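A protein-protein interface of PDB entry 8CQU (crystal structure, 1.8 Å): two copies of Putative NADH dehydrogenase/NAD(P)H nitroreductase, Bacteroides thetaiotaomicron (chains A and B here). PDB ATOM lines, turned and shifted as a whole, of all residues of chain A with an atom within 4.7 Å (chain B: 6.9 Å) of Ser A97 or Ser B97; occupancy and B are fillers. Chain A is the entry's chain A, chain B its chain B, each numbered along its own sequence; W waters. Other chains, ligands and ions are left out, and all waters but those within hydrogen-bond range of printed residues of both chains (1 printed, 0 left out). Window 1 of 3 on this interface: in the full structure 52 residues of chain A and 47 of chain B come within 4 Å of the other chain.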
ATOM      1  N   ILE A  93      24.443  25.526  12.464  1.00  0.00           N
ATOM      2  CA  ILE A  93      23.053  25.127  12.242  1.00  0.00           C
ATOM      3  C   ILE A  93      22.915  24.416  10.898  1.00  0.00           C
ATOM      4  O   ILE A  93      22.395  23.311  10.804  1.00  0.00           O
ATOM      5  CB  ILE A  93      22.085  26.281  12.427  1.00  0.00           C
ATOM      6  CG1 ILE A  93      22.102  26.855  13.858  1.00  0.00           C
ATOM      7  CG2 ILE A  93      20.691  25.828  12.044  1.00  0.00           C
ATOM      8  CD1 ILE A  93      21.421  28.252  14.013  1.00  0.00           C
ATOM      9  N   GLU A  94      23.437  25.039   9.853  1.00  0.00           N
ATOM     10  CA  GLU A  94      23.496  24.429   8.542  1.00  0.00           C
ATOM     11  C   GLU A  94      24.207  23.076   8.595  1.00  0.00           C
ATOM     12  O   GLU A  94      23.688  22.111   8.050  1.00  0.00           O
ATOM     13  CB  GLU A  94      24.243  25.320   7.550  1.00  0.00           C
ATOM     14  CG  GLU A  94      23.520  26.599   7.182  1.00  0.00           C
ATOM     15  CD  GLU A  94      23.611  27.790   8.116  1.00  0.00           C
ATOM     16  OE1 GLU A  94      23.315  28.895   7.618  1.00  0.00           O
ATOM     17  OE2 GLU A  94      23.919  27.659   9.296  1.00  0.00           O
ATOM     18  N   ASP A  95      25.356  22.982   9.271  1.00  0.00           N
ATOM     19  CA  ASP A  95      26.143  21.760   9.216  1.00  0.00           C
ATOM     20  C   ASP A  95      25.343  20.618   9.871  1.00  0.00           C
ATOM     21  O   ASP A  95      25.256  19.549   9.295  1.00  0.00           O
ATOM     22  CB  ASP A  95      27.449  21.916   9.978  1.00  0.00           C
ATOM     23  CG  ASP A  95      28.500  22.869   9.441  1.00  0.00           C
ATOM     24  OD1 ASP A  95      28.556  23.094   8.200  1.00  0.00           O
ATOM     25  OD2 ASP A  95      29.303  23.329  10.293  1.00  0.00           O
ATOM     26  N   ALA A  96      24.713  20.926  11.038  1.00  0.00           N
ATOM     27  CA  ALA A  96      23.928  19.961  11.767  1.00  0.00           C
ATOM     28  C   ALA A  96      22.642  19.550  11.043  1.00  0.00           C
ATOM     29  O   ALA A  96      22.187  18.413  11.125  1.00  0.00           O
ATOM     30  CB  ALA A  96      23.654  20.451  13.129  1.00  0.00           C
ATOM     31  N   SER A  97      22.036  20.521  10.354  1.00  0.00           N
ATOM     32  CA  SER A  97      20.854  20.293   9.551  1.00  0.00           C
ATOM     33  C   SER A  97      21.151  19.290   8.458  1.00  0.00           C
ATOM     34  O   SER A  97      20.339  18.463   8.154  1.00  0.00           O
ATOM     35  CB  SER A  97      20.335  21.597   8.942  1.00  0.00           C
ATOM     36  OG  SER A  97      19.921  22.423   9.997  1.00  0.00           O
ATOM     37  N   ILE A  98      22.247  19.553   7.746  1.00  0.00           N
ATOM     38  CA  ILE A  98      22.659  18.712   6.644  1.00  0.00           C
ATOM     39  C   ILE A  98      22.876  17.273   7.154  1.00  0.00           C
ATOM     40  O   ILE A  98      22.384  16.346   6.506  1.00  0.00           O
ATOM     41  CB  ILE A  98      23.929  19.225   5.945  1.00  0.00           C
ATOM     42  CG1 ILE A  98      23.729  20.552   5.208  1.00  0.00           C
ATOM     43  CG2 ILE A  98      24.539  18.178   5.006  1.00  0.00           C
ATOM     44  CD1 ILE A  98      25.059  21.344   4.990  1.00  0.00           C
ATOM     45  N   ALA A  99      23.660  17.099   8.232  1.00  0.00           N
ATOM     46  CA  ALA A  99      23.848  15.762   8.812  1.00  0.00           C
ATOM     47  C   ALA A  99      22.496  15.120   9.164  1.00  0.00           C
ATOM     48  O   ALA A  99      22.319  13.939   8.892  1.00  0.00           O
ATOM     49  CB  ALA A  99      24.726  15.767  10.006  1.00  0.00           C
ATOM     50  N   SER A 100      21.569  15.875   9.782  1.00  0.00           N
ATOM     51  CA  SER A 100      20.244  15.394  10.164  1.00  0.00           C
ATOM     52  C   SER A 100      19.508  14.810   8.956  1.00  0.00           C
ATOM     53  O   SER A 100      18.920  13.745   9.029  1.00  0.00           O
ATOM     54  CB  SER A 100      19.424  16.494  10.776  1.00  0.00           C
ATOM     55  OG  SER A 100      19.956  16.879  12.050  1.00  0.00           O
ATOM     56  N   ILE A 101      19.474  15.562   7.846  1.00  0.00           N
ATOM     57  CA  ILE A 101      18.675  15.130   6.701  1.00  0.00           C
ATOM     58  C   ILE A 101      19.378  13.959   6.002  1.00  0.00           C
ATOM     59  O   ILE A 101      18.724  13.076   5.450  1.00  0.00           O
ATOM     60  CB  ILE A 101      18.276  16.329   5.781  1.00  0.00           C
ATOM     61  CG1 ILE A 101      17.041  16.015   4.954  1.00  0.00           C
ATOM     62  CG2 ILE A 101      19.431  16.774   4.916  1.00  0.00           C
ATOM     63  CD1 ILE A 101      15.778  15.853   5.746  1.00  0.00           C
ATOM     64  N   TRP A 116      12.360  13.805  12.359  1.00  0.00           N
ATOM     65  CA  TRP A 116      13.232  14.835  12.909  1.00  0.00           C
ATOM     66  C   TRP A 116      12.473  15.485  14.037  1.00  0.00           C
ATOM     67  O   TRP A 116      11.408  16.043  13.813  1.00  0.00           O
ATOM     68  CB  TRP A 116      13.583  15.810  11.786  1.00  0.00           C
ATOM     69  CG  TRP A 116      14.347  17.059  12.141  1.00  0.00           C
ATOM     70  CD1 TRP A 116      14.145  17.921  13.189  1.00  0.00           C
ATOM     71  CD2 TRP A 116      15.324  17.693  11.306  1.00  0.00           C
ATOM     72  NE1 TRP A 116      14.938  19.026  13.072  1.00  0.00           N
ATOM     73  CE2 TRP A 116      15.690  18.904  11.938  1.00  0.00           C
ATOM     74  CE3 TRP A 116      15.865  17.377  10.055  1.00  0.00           C
ATOM     75  CZ2 TRP A 116      16.635  19.782  11.399  1.00  0.00           C
ATOM     76  CZ3 TRP A 116      16.808  18.239   9.528  1.00  0.00           C
ATOM     77  CH2 TRP A 116      17.177  19.414  10.190  1.00  0.00           C
ATOM     78  N   LEU A 147      20.978  20.370  17.838  1.00  0.00           N
ATOM     79  CA  LEU A 147      19.989  20.760  16.825  1.00  0.00           C
ATOM     80  C   LEU A 147      18.706  19.937  16.919  1.00  0.00           C
ATOM     81  O   LEU A 147      17.594  20.471  16.786  1.00  0.00           O
ATOM     82  CB  LEU A 147      20.584  20.563  15.428  1.00  0.00           C
ATOM     83  CG  LEU A 147      19.690  21.199  14.365  1.00  0.00           C
ATOM     84  CD1 LEU A 147      19.843  22.718  14.399  1.00  0.00           C
ATOM     85  CD2 LEU A 147      19.920  20.678  12.991  1.00  0.00           C
ATOM     86  N   TRP B  48      10.424  28.565   2.648  1.00  0.00           N
ATOM     87  CA  TRP B  48      11.422  28.838   1.644  1.00  0.00           C
ATOM     88  C   TRP B  48      10.820  29.417   0.388  1.00  0.00           C
ATOM     89  O   TRP B  48       9.632  29.237   0.092  1.00  0.00           O
ATOM     90  CB  TRP B  48      12.376  27.652   1.338  1.00  0.00           C
ATOM     91  CG  TRP B  48      11.813  26.268   1.619  1.00  0.00           C
ATOM     92  CD1 TRP B  48      12.267  25.370   2.546  1.00  0.00           C
ATOM     93  CD2 TRP B  48      10.688  25.637   1.005  1.00  0.00           C
ATOM     94  NE1 TRP B  48      11.480  24.269   2.558  1.00  0.00           N
ATOM     95  CE2 TRP B  48      10.559  24.357   1.590  1.00  0.00           C
ATOM     96  CE3 TRP B  48       9.829  25.964  -0.044  1.00  0.00           C
ATOM     97  CZ2 TRP B  48       9.590  23.446   1.213  1.00  0.00           C
ATOM     98  CZ3 TRP B  48       8.869  25.045  -0.431  1.00  0.00           C
ATOM     99  CH2 TRP B  48       8.727  23.835   0.221  1.00  0.00           C
ATOM    100  N   VAL B  82      18.526  30.095  -2.345  1.00  0.00           N
ATOM    101  CA  VAL B  82      17.615  29.545  -1.372  1.00  0.00           C
ATOM    102  C   VAL B  82      17.459  30.587  -0.281  1.00  0.00           C
ATOM    103  O   VAL B  82      18.466  31.077   0.279  1.00  0.00           O
ATOM    104  CB  VAL B  82      18.160  28.234  -0.778  1.00  0.00           C
ATOM    105  CG1 VAL B  82      17.260  27.682   0.308  1.00  0.00           C
ATOM    106  CG2 VAL B  82      18.449  27.193  -1.877  1.00  0.00           C
ATOM    107  N   VAL B  91      12.619  28.148  12.536  1.00  0.00           N
ATOM    108  CA  VAL B  91      13.667  27.226  12.132  1.00  0.00           C
ATOM    109  C   VAL B  91      13.839  27.287  10.609  1.00  0.00           C
ATOM    110  O   VAL B  91      14.157  26.302   9.957  1.00  0.00           O
ATOM    111  CB  VAL B  91      13.365  25.838  12.676  1.00  0.00           C
ATOM    112  CG1 VAL B  91      13.462  25.799  14.252  1.00  0.00           C
ATOM    113  CG2 VAL B  91      12.034  25.292  12.255  1.00  0.00           C
ATOM    114  N   TRP B  92      13.722  28.491  10.071  1.00  0.00           N
ATOM    115  CA  TRP B  92      13.931  28.744   8.656  1.00  0.00           C
ATOM    116  C   TRP B  92      15.328  28.326   8.191  1.00  0.00           C
ATOM    117  O   TRP B  92      15.461  27.872   7.068  1.00  0.00           O
ATOM    118  CB  TRP B  92      13.601  30.195   8.312  1.00  0.00           C
ATOM    119  CG  TRP B  92      14.615  31.171   8.814  1.00  0.00           C
ATOM    120  CD1 TRP B  92      14.510  31.926   9.939  1.00  0.00           C
ATOM    121  CD2 TRP B  92      15.776  31.622   8.126  1.00  0.00           C
ATOM    122  NE1 TRP B  92      15.610  32.703  10.079  1.00  0.00           N
ATOM    123  CE2 TRP B  92      16.371  32.594   8.945  1.00  0.00           C
ATOM    124  CE3 TRP B  92      16.384  31.296   6.905  1.00  0.00           C
ATOM    125  CZ2 TRP B  92      17.585  33.201   8.639  1.00  0.00           C
ATOM    126  CZ3 TRP B  92      17.582  31.926   6.586  1.00  0.00           C
ATOM    127  CH2 TRP B  92      18.167  32.867   7.435  1.00  0.00           C
ATOM    128  N   ILE B  93      16.353  28.430   9.041  1.00  0.00           N
ATOM    129  CA  ILE B  93      17.671  28.022   8.665  1.00  0.00           C
ATOM    130  C   ILE B  93      17.704  26.522   8.402  1.00  0.00           C
ATOM    131  O   ILE B  93      18.234  26.055   7.387  1.00  0.00           O
ATOM    132  CB  ILE B  93      18.749  28.493   9.693  1.00  0.00           C
ATOM    133  CG1 ILE B  93      18.773  30.004   9.900  1.00  0.00           C
ATOM    134  CG2 ILE B  93      20.112  28.002   9.321  1.00  0.00           C
ATOM    135  CD1 ILE B  93      19.418  30.450  11.203  1.00  0.00           C
ATOM    136  N   GLU B  94      17.212  25.769   9.359  1.00  0.00           N
ATOM    137  CA  GLU B  94      17.067  24.312   9.192  1.00  0.00           C
ATOM    138  C   GLU B  94      16.309  23.942   7.907  1.00  0.00           C
ATOM    139  O   GLU B  94      16.802  23.130   7.115  1.00  0.00           O
ATOM    140  CB  GLU B  94      16.385  23.649  10.400  1.00  0.00           C
ATOM    141  CG  GLU B  94      17.208  23.731  11.678  1.00  0.00           C
ATOM    142  CD  GLU B  94      17.077  24.971  12.559  1.00  0.00           C
ATOM    143  OE1 GLU B  94      17.192  24.834  13.808  1.00  0.00           O
ATOM    144  OE2 GLU B  94      16.752  26.079  12.020  1.00  0.00           O
ATOM    145  N   ASP B  95      15.191  24.592   7.656  1.00  0.00           N
ATOM    146  CA  ASP B  95      14.303  24.292   6.545  1.00  0.00           C
ATOM    147  C   ASP B  95      15.039  24.628   5.230  1.00  0.00           C
ATOM    148  O   ASP B  95      14.992  23.887   4.287  1.00  0.00           O
ATOM    149  CB  ASP B  95      13.022  25.143   6.584  1.00  0.00           C
ATOM    150  CG  ASP B  95      11.982  24.917   7.722  1.00  0.00           C
ATOM    151  OD1 ASP B  95      11.930  23.807   8.267  1.00  0.00           O
ATOM    152  OD2 ASP B  95      11.153  25.898   8.027  1.00  0.00           O
ATOM    153  N   ALA B  96      15.737  25.741   5.161  1.00  0.00           N
ATOM    154  CA  ALA B  96      16.439  26.140   3.944  1.00  0.00           C
ATOM    155  C   ALA B  96      17.651  25.258   3.662  1.00  0.00           C
ATOM    156  O   ALA B  96      18.079  25.048   2.483  1.00  0.00           O
ATOM    157  CB  ALA B  96      16.832  27.609   4.056  1.00  0.00           C
ATOM    158  N   SER B  97      18.342  24.900   4.731  1.00  0.00           N
ATOM    159  CA  SER B  97      19.462  23.968   4.629  1.00  0.00           C
ATOM    160  C   SER B  97      19.018  22.628   4.038  1.00  0.00           C
ATOM    161  O   SER B  97      19.717  22.038   3.219  1.00  0.00           O
ATOM    162  CB  SER B  97      20.069  23.707   5.962  1.00  0.00           C
ATOM    163  OG  SER B  97      20.583  24.883   6.579  1.00  0.00           O
ATOM    164  N   ILE B  98      17.889  22.112   4.553  1.00  0.00           N
ATOM    165  CA  ILE B  98      17.281  20.881   4.034  1.00  0.00           C
ATOM    166  C   ILE B  98      17.009  21.034   2.548  1.00  0.00           C
ATOM    167  O   ILE B  98      17.330  20.138   1.778  1.00  0.00           O
ATOM    168  CB  ILE B  98      15.988  20.470   4.758  1.00  0.00           C
ATOM    169  CG1 ILE B  98      16.251  20.109   6.209  1.00  0.00           C
ATOM    170  CG2 ILE B  98      15.243  19.364   4.010  1.00  0.00           C
ATOM    171  CD1 ILE B  98      15.024  19.937   7.021  1.00  0.00           C
ATOM    172  N   ALA B  99      16.371  22.151   2.166  1.00  0.00           N
ATOM    173  CA  ALA B  99      16.010  22.363   0.775  1.00  0.00           C
ATOM    174  C   ALA B  99      17.286  22.445  -0.094  1.00  0.00           C
ATOM    175  O   ALA B  99      17.287  21.886  -1.168  1.00  0.00           O
ATOM    176  CB  ALA B  99      15.138  23.591   0.696  1.00  0.00           C
ATOM    177  N   SER B 100      18.372  23.033   0.424  1.00  0.00           N
ATOM    178  CA  SER B 100      19.651  23.172  -0.265  1.00  0.00           C
ATOM    179  C   SER B 100      20.232  21.821  -0.601  1.00  0.00           C
ATOM    180  O   SER B 100      20.749  21.590  -1.680  1.00  0.00           O
ATOM    181  CB  SER B 100      20.625  24.017   0.572  1.00  0.00           C
ATOM    182  OG  SER B 100      20.184  25.363   0.614  1.00  0.00           O
ATOM    183  N   ILE B 101      20.229  20.951   0.399  1.00  0.00           N
ATOM    184  CA  ILE B 101      20.733  19.595   0.255  1.00  0.00           C
ATOM    185  C   ILE B 101      19.927  18.768  -0.702  1.00  0.00           C
ATOM    186  O   ILE B 101      20.520  17.989  -1.480  1.00  0.00           O
ATOM    187  CB  ILE B 101      20.777  18.919   1.652  1.00  0.00           C
ATOM    188  CG1 ILE B 101      22.135  19.297   2.203  1.00  0.00           C
ATOM    189  CG2 ILE B 101      20.591  17.424   1.627  1.00  0.00           C
ATOM    190  CD1 ILE B 101      23.379  18.733   1.440  1.00  0.00           C
ATOM    191  N   MET B 102      18.592  18.915  -0.622  1.00  0.00           N
ATOM    192  CA  MET B 102      17.728  18.164  -1.528  1.00  0.00           C
ATOM    193  C   MET B 102      18.074  18.561  -2.971  1.00  0.00           C
ATOM    194  O   MET B 102      18.165  17.673  -3.837  1.00  0.00           O
ATOM    195  CB  MET B 102      16.245  18.493  -1.290  1.00  0.00           C
ATOM    196  CG  MET B 102      15.728  18.051   0.044  1.00  0.00           C
ATOM    197  SD  MET B 102      15.676  16.271   0.108  1.00  0.00           S
ATOM    198  CE  MET B 102      14.668  16.040   1.561  1.00  0.00           C
ATOM    199  N   TRP B 116      27.534  24.257  -2.983  1.00  0.00           N
ATOM    200  CA  TRP B 116      26.850  25.109  -2.030  1.00  0.00           C
ATOM    201  C   TRP B 116      27.756  26.296  -1.698  1.00  0.00           C
ATOM    202  O   TRP B 116      28.888  26.149  -1.188  1.00  0.00           O
ATOM    203  CB  TRP B 116      26.491  24.223  -0.832  1.00  0.00           C
ATOM    204  CG  TRP B 116      25.939  24.920   0.361  1.00  0.00           C
ATOM    205  CD1 TRP B 116      26.327  26.101   0.932  1.00  0.00           C
ATOM    206  CD2 TRP B 116      24.978  24.352   1.256  1.00  0.00           C
ATOM    207  NE1 TRP B 116      25.564  26.350   2.040  1.00  0.00           N
ATOM    208  CE2 TRP B 116      24.724  25.314   2.247  1.00  0.00           C
ATOM    209  CE3 TRP B 116      24.211  23.177   1.216  1.00  0.00           C
ATOM    210  CZ2 TRP B 116      23.868  25.064   3.305  1.00  0.00           C
ATOM    211  CZ3 TRP B 116      23.353  22.944   2.257  1.00  0.00           C
ATOM    212  CH2 TRP B 116      23.186  23.862   3.286  1.00  0.00           C
ATOM    213  N   GLN B 118      27.779  29.377   0.706  1.00  0.00           N
ATOM    214  CA  GLN B 118      27.095  29.828   1.903  1.00  0.00           C
ATOM    215  C   GLN B 118      26.904  31.378   1.835  1.00  0.00           C
ATOM    216  O   GLN B 118      27.837  32.091   1.611  1.00  0.00           O
ATOM    217  CB  GLN B 118      27.972  29.434   3.085  1.00  0.00           C
ATOM    218  CG  GLN B 118      27.364  29.915   4.419  1.00  0.00           C
ATOM    219  CD  GLN B 118      26.062  29.247   4.800  1.00  0.00           C
ATOM    220  OE1 GLN B 118      25.808  28.120   4.394  1.00  0.00           O
ATOM    221  NE2 GLN B 118      25.246  29.873   5.668  1.00  0.00           N
ATOM    222  N   ARG B 120      24.299  33.041   4.374  1.00  0.00           N
ATOM    223  CA  ARG B 120      24.060  33.492   5.748  1.00  0.00           C
ATOM    224  C   ARG B 120      25.392  33.511   6.512  1.00  0.00           C
ATOM    225  O   ARG B 120      26.188  32.555   6.394  1.00  0.00           O
ATOM    226  CB  ARG B 120      23.005  32.620   6.408  1.00  0.00           C
ATOM    227  CG  ARG B 120      22.531  33.205   7.740  1.00  0.00           C
ATOM    228  CD  ARG B 120      21.671  32.137   8.396  1.00  0.00           C
ATOM    229  NE  ARG B 120      22.451  31.049   8.980  1.00  0.00           N
ATOM    230  CZ  ARG B 120      22.973  31.053  10.223  1.00  0.00           C
ATOM    231  NH1 ARG B 120      22.757  32.087  11.041  1.00  0.00           N
ATOM    232  NH2 ARG B 120      23.667  30.015  10.650  1.00  0.00           N
ATOM    233  N   LEU B 147      19.911  32.024   2.592  1.00  0.00           N
ATOM    234  CA  LEU B 147      20.795  31.017   3.156  1.00  0.00           C
ATOM    235  C   LEU B 147      22.027  30.786   2.258  1.00  0.00           C
ATOM    236  O   LEU B 147      23.155  30.743   2.755  1.00  0.00           O
ATOM    237  CB  LEU B 147      20.075  29.686   3.259  1.00  0.00           C
ATOM    238  CG  LEU B 147      20.865  28.712   4.136  1.00  0.00           C
ATOM    239  CD1 LEU B 147      20.611  29.009   5.597  1.00  0.00           C
ATOM    240  CD2 LEU B 147      20.559  27.316   3.858  1.00  0.00           C
ATOM    241  N   SER B 148      21.776  30.483   0.986  1.00  0.00           N
ATOM    242  CA  SER B 148      22.781  29.851   0.165  1.00  0.00           C
ATOM    243  C   SER B 148      22.499  30.122  -1.293  1.00  0.00           C
ATOM    244  O   SER B 148      21.360  30.415  -1.671  1.00  0.00           O
ATOM    245  CB  SER B 148      22.780  28.305   0.390  1.00  0.00           C
ATOM    246  OG  SER B 148      21.534  27.742   0.017  1.00  0.00           O
HETATM  247  O   HOH W   1      24.742  28.677  13.097  1.00  0.00           O
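Ser A97 touches two residues of chain B.
Ser B97 touches two residues of chain A.
Printed residues of chain B within 4 Å of Glu A94: Ile B93 (3.7 Å), Ser B97 (3.5 Å), Gln B118 (2.9 Å), Arg B120 (2.7 Å) and Leu B147 (3.4 Å).
Of the printed residues of chain A, Leu B147 touches Glu A94 (3.4 Å).
Printed residues of chain B within 4 Å of Ile A101: Ile B98 and Ile B101.
The nearest printed residue of chain A that does not touch Ser B97 is Ile A98 (4.7 Å).
Ile A93 touches Glu B94, and with the chains exchanged Glu A94 touches Ile B93.
Glu A94 touches Leu B147, and with the chains exchanged Leu A147 touches Glu B94.
Ser B97 touches its own counterpart, Ser A97.
Ile A98 touches Ile B101, and with the chains exchanged Ile A101 touches Ile B98.
Of the 15 pairs that touch across the chains among the printed residues, 13 have their exchanged pair printed and touching as well.
Water W1 lies within hydrogen-bond range of NH2 of Arg B120 and N of Ile A93.
Printed residues of chain A that touch a printed residue of chain B: Ile A93, Glu A94, Ser A97, Ile A98, Ile A101, Trp A116 and Leu A147.
Hydrophobic or aromatic side chains of chain B that line the printed part of chain A: Ile B93, Ile B98, Ile B101, Trp B116 and Leu B147.
Among the printed residues, 15 pairs touch across the chains.
The side-chain carboxylate (OE1) of Glu A94 is in salt-bridge range of the guanidinium group (NE) of Arg B120, at 2.7 Å.
The side-chain carboxylate (OE1) of Glu A94 lies within hydrogen-bond range of the side-chain amide nitrogen (NE2) of Gln B118 (2.9 Å).
Among the printed residues, merely in contact across the chains: Ile A93 with Ile B93 (3.5 Å), Ile A93 with Glu B94 (3.7 Å), Glu A94 with Ile B93 (3.7 Å), Glu A94 with Ser B97 (3.5 Å), Glu A94 with Leu B147 (3.4 Å), Ser A97 with Glu B94 (3.4 Å), Ser A97 with Ser B97 (3.7 Å), Ile A98 with Ile B101 (3.6 Å), Ile A98 with Trp B116 (3.6 Å), Ile A101 with Ile B98 (3.9 Å), Ile A101 with Ile B101 (3.5 Å), Trp A116 with Ile B98 (3.5 Å) and Leu A147 with Glu B94 (3.4 Å).
NE2 of Gln B118 is in hydrogen-bond range of O of Arg B120 (2.9 Å).
OG of Ser B97 sits at hydrogen-bond distance from O of Ile B93.
The backbone NH (N) of Leu B147 lies within hydrogen-bond range of the backbone carbonyl oxygen (O) of Val B82 (2.9 Å).
The indole nitrogen (NE1) of Trp B116 lies within hydrogen-bond range of the side-chain amide oxygen (OE1) of Gln B118, at 3.0 Å.
OG of Ser A97 sits at hydrogen-bond distance from O of Ile A93.
N of Arg B120 sits at hydrogen-bond distance from O of Leu B147.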
